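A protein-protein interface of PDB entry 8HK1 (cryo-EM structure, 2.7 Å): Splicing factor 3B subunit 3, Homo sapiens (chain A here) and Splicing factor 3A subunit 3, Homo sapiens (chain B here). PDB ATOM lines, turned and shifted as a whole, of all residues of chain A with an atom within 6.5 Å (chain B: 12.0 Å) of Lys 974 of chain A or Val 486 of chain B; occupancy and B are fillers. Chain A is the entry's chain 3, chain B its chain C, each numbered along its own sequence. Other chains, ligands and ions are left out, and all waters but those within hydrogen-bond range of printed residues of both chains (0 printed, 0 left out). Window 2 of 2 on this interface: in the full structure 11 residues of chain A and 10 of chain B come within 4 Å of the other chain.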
ATOM      1  N   LEU A 940     -33.529  13.260 -10.282  1.00  0.00           N
ATOM      2  CA  LEU A 940     -33.347  14.207 -11.378  1.00  0.00           C
ATOM      3  C   LEU A 940     -31.997  14.914 -11.307  1.00  0.00           C
ATOM      4  O   LEU A 940     -31.216  14.814 -12.255  1.00  0.00           O
ATOM      5  CB  LEU A 940     -34.494  15.222 -11.388  1.00  0.00           C
ATOM      6  CG  LEU A 940     -34.606  16.086 -12.645  1.00  0.00           C
ATOM      7  CD1 LEU A 940     -35.188  15.282 -13.791  1.00  0.00           C
ATOM      8  CD2 LEU A 940     -35.449  17.319 -12.378  1.00  0.00           C
ATOM      9  N   HIS A 941     -31.687  15.604 -10.210  1.00  0.00           N
ATOM     10  CA  HIS A 941     -30.354  16.162 -10.011  1.00  0.00           C
ATOM     11  C   HIS A 941     -30.171  16.486  -8.530  1.00  0.00           C
ATOM     12  O   HIS A 941     -31.032  16.182  -7.699  1.00  0.00           O
ATOM     13  CB  HIS A 941     -30.106  17.387 -10.904  1.00  0.00           C
ATOM     14  CG  HIS A 941     -31.200  18.407 -10.870  1.00  0.00           C
ATOM     15  ND1 HIS A 941     -32.070  18.598 -11.921  1.00  0.00           N
ATOM     16  CD2 HIS A 941     -31.553  19.306  -9.922  1.00  0.00           C
ATOM     17  CE1 HIS A 941     -32.914  19.571 -11.620  1.00  0.00           C
ATOM     18  NE2 HIS A 941     -32.624  20.014 -10.413  1.00  0.00           N
ATOM     19  N   LEU A 972     -36.826  25.769 -10.999  1.00  0.00           N
ATOM     20  CA  LEU A 972     -36.359  24.480 -11.492  1.00  0.00           C
ATOM     21  C   LEU A 972     -35.567  24.655 -12.782  1.00  0.00           C
ATOM     22  O   LEU A 972     -35.979  25.390 -13.681  1.00  0.00           O
ATOM     23  CB  LEU A 972     -37.539  23.538 -11.724  1.00  0.00           C
ATOM     24  CG  LEU A 972     -37.175  22.088 -12.056  1.00  0.00           C
ATOM     25  CD1 LEU A 972     -36.272  21.504 -10.989  1.00  0.00           C
ATOM     26  CD2 LEU A 972     -38.423  21.241 -12.230  1.00  0.00           C
ATOM     27  N   GLY A 973     -34.418  23.977 -12.864  1.00  0.00           N
ATOM     28  CA  GLY A 973     -33.598  23.980 -14.052  1.00  0.00           C
ATOM     29  C   GLY A 973     -33.405  22.567 -14.580  1.00  0.00           C
ATOM     30  O   GLY A 973     -33.892  21.585 -14.010  1.00  0.00           O
ATOM     31  N   LYS A 974     -32.676  22.477 -15.692  1.00  0.00           N
ATOM     32  CA  LYS A 974     -32.427  21.184 -16.313  1.00  0.00           C
ATOM     33  C   LYS A 974     -31.304  20.403 -15.648  1.00  0.00           C
ATOM     34  O   LYS A 974     -31.274  19.177 -15.784  1.00  0.00           O
ATOM     35  CB  LYS A 974     -32.120  21.365 -17.799  1.00  0.00           C
ATOM     36  CG  LYS A 974     -33.309  21.830 -18.620  1.00  0.00           C
ATOM     37  CD  LYS A 974     -33.773  20.753 -19.586  1.00  0.00           C
ATOM     38  CE  LYS A 974     -35.290  20.707 -19.673  1.00  0.00           C
ATOM     39  NZ  LYS A 974     -35.783  19.384 -20.146  1.00  0.00           N
ATOM     40  N   LYS A 975     -30.390  21.062 -14.936  1.00  0.00           N
ATOM     41  CA  LYS A 975     -29.272  20.358 -14.322  1.00  0.00           C
ATOM     42  C   LYS A 975     -29.152  20.657 -12.833  1.00  0.00           C
ATOM     43  O   LYS A 975     -28.442  19.947 -12.115  1.00  0.00           O
ATOM     44  CB  LYS A 975     -27.964  20.712 -15.031  1.00  0.00           C
ATOM     45  CG  LYS A 975     -27.845  20.144 -16.431  1.00  0.00           C
ATOM     46  CD  LYS A 975     -26.842  19.003 -16.474  1.00  0.00           C
ATOM     47  CE  LYS A 975     -26.171  18.904 -17.833  1.00  0.00           C
ATOM     48  NZ  LYS A 975     -25.239  20.036 -18.067  1.00  0.00           N
ATOM     49  N   LYS A 976     -29.833  21.697 -12.363  1.00  0.00           N
ATOM     50  CA  LYS A 976     -29.803  22.070 -10.953  1.00  0.00           C
ATOM     51  C   LYS A 976     -30.902  23.098 -10.705  1.00  0.00           C
ATOM     52  O   LYS A 976     -31.687  23.409 -11.607  1.00  0.00           O
ATOM     53  CB  LYS A 976     -28.410  22.590 -10.560  1.00  0.00           C
ATOM     54  CG  LYS A 976     -28.007  23.880 -11.246  1.00  0.00           C
ATOM     55  CD  LYS A 976     -26.747  24.449 -10.624  1.00  0.00           C
ATOM     56  CE  LYS A 976     -26.415  25.819 -11.184  1.00  0.00           C
ATOM     57  NZ  LYS A 976     -25.134  26.346 -10.640  1.00  0.00           N
ATOM     58  N   LEU A 978     -31.961  26.973  -9.854  1.00  0.00           N
ATOM     59  CA  LEU A 978     -31.425  28.275 -10.245  1.00  0.00           C
ATOM     60  C   LEU A 978     -31.823  29.308  -9.197  1.00  0.00           C
ATOM     61  O   LEU A 978     -33.014  29.530  -8.954  1.00  0.00           O
ATOM     62  CB  LEU A 978     -31.928  28.664 -11.630  1.00  0.00           C
ATOM     63  CG  LEU A 978     -31.613  27.660 -12.739  1.00  0.00           C
ATOM     64  CD1 LEU A 978     -32.365  28.012 -14.006  1.00  0.00           C
ATOM     65  CD2 LEU A 978     -30.119  27.595 -13.001  1.00  0.00           C
ATOM     66  N   GLU B 478     -28.700  32.858 -11.442  1.00  0.00           N
ATOM     67  CA  GLU B 478     -28.419  31.611 -12.147  1.00  0.00           C
ATOM     68  C   GLU B 478     -29.386  31.514 -13.319  1.00  0.00           C
ATOM     69  O   GLU B 478     -30.557  31.169 -13.143  1.00  0.00           O
ATOM     70  CB  GLU B 478     -28.543  30.411 -11.217  1.00  0.00           C
ATOM     71  N   TYR B 479     -28.897  31.839 -14.512  1.00  0.00           N
ATOM     72  CA  TYR B 479     -29.664  31.633 -15.729  1.00  0.00           C
ATOM     73  C   TYR B 479     -29.094  30.443 -16.490  1.00  0.00           C
ATOM     74  O   TYR B 479     -27.888  30.192 -16.450  1.00  0.00           O
ATOM     75  CB  TYR B 479     -29.638  32.888 -16.600  1.00  0.00           C
ATOM     76  N   GLU B 480     -29.968  29.712 -17.175  1.00  0.00           N
ATOM     77  CA  GLU B 480     -29.583  28.586 -18.025  1.00  0.00           C
ATOM     78  C   GLU B 480     -30.142  28.872 -19.412  1.00  0.00           C
ATOM     79  O   GLU B 480     -31.327  28.664 -19.678  1.00  0.00           O
ATOM     80  CB  GLU B 480     -30.097  27.253 -17.458  1.00  0.00           C
ATOM     81  N   ASP B 481     -29.281  29.367 -20.297  1.00  0.00           N
ATOM     82  CA  ASP B 481     -29.721  29.798 -21.612  1.00  0.00           C
ATOM     83  C   ASP B 481     -30.190  28.605 -22.445  1.00  0.00           C
ATOM     84  O   ASP B 481     -29.835  27.451 -22.197  1.00  0.00           O
ATOM     85  CB  ASP B 481     -28.601  30.542 -22.338  1.00  0.00           C
ATOM     86  N   SER B 482     -31.001  28.909 -23.460  1.00  0.00           N
ATOM     87  CA  SER B 482     -31.551  27.903 -24.361  1.00  0.00           C
ATOM     88  C   SER B 482     -30.616  27.581 -25.521  1.00  0.00           C
ATOM     89  O   SER B 482     -31.067  27.052 -26.546  1.00  0.00           O
ATOM     90  CB  SER B 482     -32.916  28.354 -24.882  1.00  0.00           C
ATOM     91  N   SER B 483     -29.326  27.899 -25.395  1.00  0.00           N
ATOM     92  CA  SER B 483     -28.359  27.501 -26.411  1.00  0.00           C
ATOM     93  C   SER B 483     -28.246  25.988 -26.519  1.00  0.00           C
ATOM     94  O   SER B 483     -28.355  25.446 -27.626  1.00  0.00           O
ATOM     95  CB  SER B 483     -26.990  28.110 -26.103  1.00  0.00           C
ATOM     96  N   GLY B 484     -28.033  25.297 -25.402  1.00  0.00           N
ATOM     97  CA  GLY B 484     -28.128  23.854 -25.369  1.00  0.00           C
ATOM     98  C   GLY B 484     -29.437  23.429 -24.739  1.00  0.00           C
ATOM     99  O   GLY B 484     -29.956  22.343 -25.015  1.00  0.00           O
ATOM    100  N   ASN B 485     -29.968  24.288 -23.870  1.00  0.00           N
ATOM    101  CA  ASN B 485     -31.259  24.206 -23.200  1.00  0.00           C
ATOM    102  C   ASN B 485     -31.312  23.082 -22.167  1.00  0.00           C
ATOM    103  O   ASN B 485     -32.324  22.951 -21.479  1.00  0.00           O
ATOM    104  CB  ASN B 485     -32.441  24.036 -24.176  1.00  0.00           C
ATOM    105  N   VAL B 486     -30.264  22.271 -22.025  1.00  0.00           N
ATOM    106  CA  VAL B 486     -30.246  21.212 -21.023  1.00  0.00           C
ATOM    107  C   VAL B 486     -28.901  21.219 -20.311  1.00  0.00           C
ATOM    108  O   VAL B 486     -28.591  20.304 -19.538  1.00  0.00           O
ATOM    109  CB  VAL B 486     -30.528  19.837 -21.655  1.00  0.00           C
ATOM    110  N   VAL B 487     -28.093  22.246 -20.569  1.00  0.00           N
ATOM    111  CA  VAL B 487     -26.757  22.352 -19.999  1.00  0.00           C
ATOM    112  C   VAL B 487     -26.460  23.818 -19.724  1.00  0.00           C
ATOM    113  O   VAL B 487     -27.294  24.695 -19.968  1.00  0.00           O
ATOM    114  CB  VAL B 487     -25.683  21.736 -20.927  1.00  0.00           C
ATOM    115  N   ASN B 488     -25.260  24.073 -19.197  1.00  0.00           N
ATOM    116  CA  ASN B 488     -24.732  25.424 -19.037  1.00  0.00           C
ATOM    117  C   ASN B 488     -25.613  26.300 -18.157  1.00  0.00           C
ATOM    118  O   ASN B 488     -26.173  27.298 -18.623  1.00  0.00           O
ATOM    119  CB  ASN B 488     -24.541  26.084 -20.407  1.00  0.00           C
ATOM    120  N   LYS B 489     -25.748  25.934 -16.881  1.00  0.00           N
ATOM    121  CA  LYS B 489     -26.459  26.780 -15.931  1.00  0.00           C
ATOM    122  C   LYS B 489     -25.538  27.797 -15.269  1.00  0.00           C
ATOM    123  O   LYS B 489     -25.989  28.531 -14.379  1.00  0.00           O
ATOM    124  CB  LYS B 489     -27.153  25.931 -14.859  1.00  0.00           C
ATOM    125  N   LYS B 490     -24.265  27.863 -15.668  1.00  0.00           N
ATOM    126  CA  LYS B 490     -23.330  28.821 -15.088  1.00  0.00           C
ATOM    127  C   LYS B 490     -23.391  30.186 -15.756  1.00  0.00           C
ATOM    128  O   LYS B 490     -22.504  31.012 -15.517  1.00  0.00           O
ATOM    129  CB  LYS B 490     -21.904  28.273 -15.167  1.00  0.00           C
ATOM    130  N   THR B 491     -24.401  30.442 -16.583  1.00  0.00           N
ATOM    131  CA  THR B 491     -24.521  31.730 -17.254  1.00  0.00           C
ATOM    132  C   THR B 491     -24.928  32.806 -16.257  1.00  0.00           C
ATOM    133  O   THR B 491     -25.862  32.615 -15.470  1.00  0.00           O
ATOM    134  CB  THR B 491     -25.538  31.640 -18.389  1.00  0.00           C
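Lys 974 of chain A touches just these residues of chain B: Asn 485 and Val 486.
Val 486 of chain B touches just these residues of chain A: Lys 974 (3.7 Å) and Lys 975 (3.2 Å).
No residue of chain B comes within 4 Å of Leu 972 of chain A.
Gly 973 of chain A touches none of the printed residues of chain B.
Lys 975 of chain A touches just these residues of chain B: Val 486 (3.2 Å) and Val 487 (3.4 Å).
Printed residues of chain B within 4 Å of Leu 978 of chain A: Glu 478 and Lys 489.
Of the printed residues of chain A, Val 487 of chain B touches Lys 975.
Of the printed residues of chain A, Asn 485 of chain B touches Lys 974 (3.2 Å).
Of the printed residues of chain A, Lys 489 of chain B touches Lys 976 (3.8 Å) and Leu 978 (3.9 Å).
The nearest residue of chain B that does not touch Lys 974 of chain A is Val 487 of chain B (5.0 Å).
The nearest printed residue of chain A that does not touch Val 486 of chain B is Gly 973 of chain A (7.3 Å).
The nearest printed residue of chain B that does not touch Leu 978 of chain A is Glu 480 of chain B (4.2 Å).
Asn 485 of chain B touches Lys 974 of chain A.
Lys 974 of chain A touches Val 486 of chain B (CB to CA, 3.7 Å).
Val 486 of chain B touches Lys 975 of chain A.
Val 487 of chain B touches Lys 975 of chain A (CB to NZ, 3.4 Å).
CE of Lys 976 of chain A touches CB of Lys 489 of chain B, 3.8 Å away.
CB of Leu 978 of chain A touches O of Glu 478 of chain B, 3.2 Å away.
Lys 489 of chain B touches Leu 978 of chain A.
Of the 14 printed residues of chain B, 5 touch a printed residue of chain A.
Printed residues of chain B that touch a printed residue of chain A: Glu 478, Asn 485, Val 486, Val 487 and Lys 489.
Hydrophobic or aromatic side chains of chain B that line the printed part of chain A: Val 486 and Val 487.
Of the 8 printed residues of chain A, 4 touch a printed residue of chain B.
Hydrophobic or aromatic side chains of chain A within 4 Å of the printed part of chain B: Leu 978.
Among the printed residues, no Asp or Glu carboxylate lies within 4 Å of a Lys or Arg side-chain nitrogen of the other chain.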
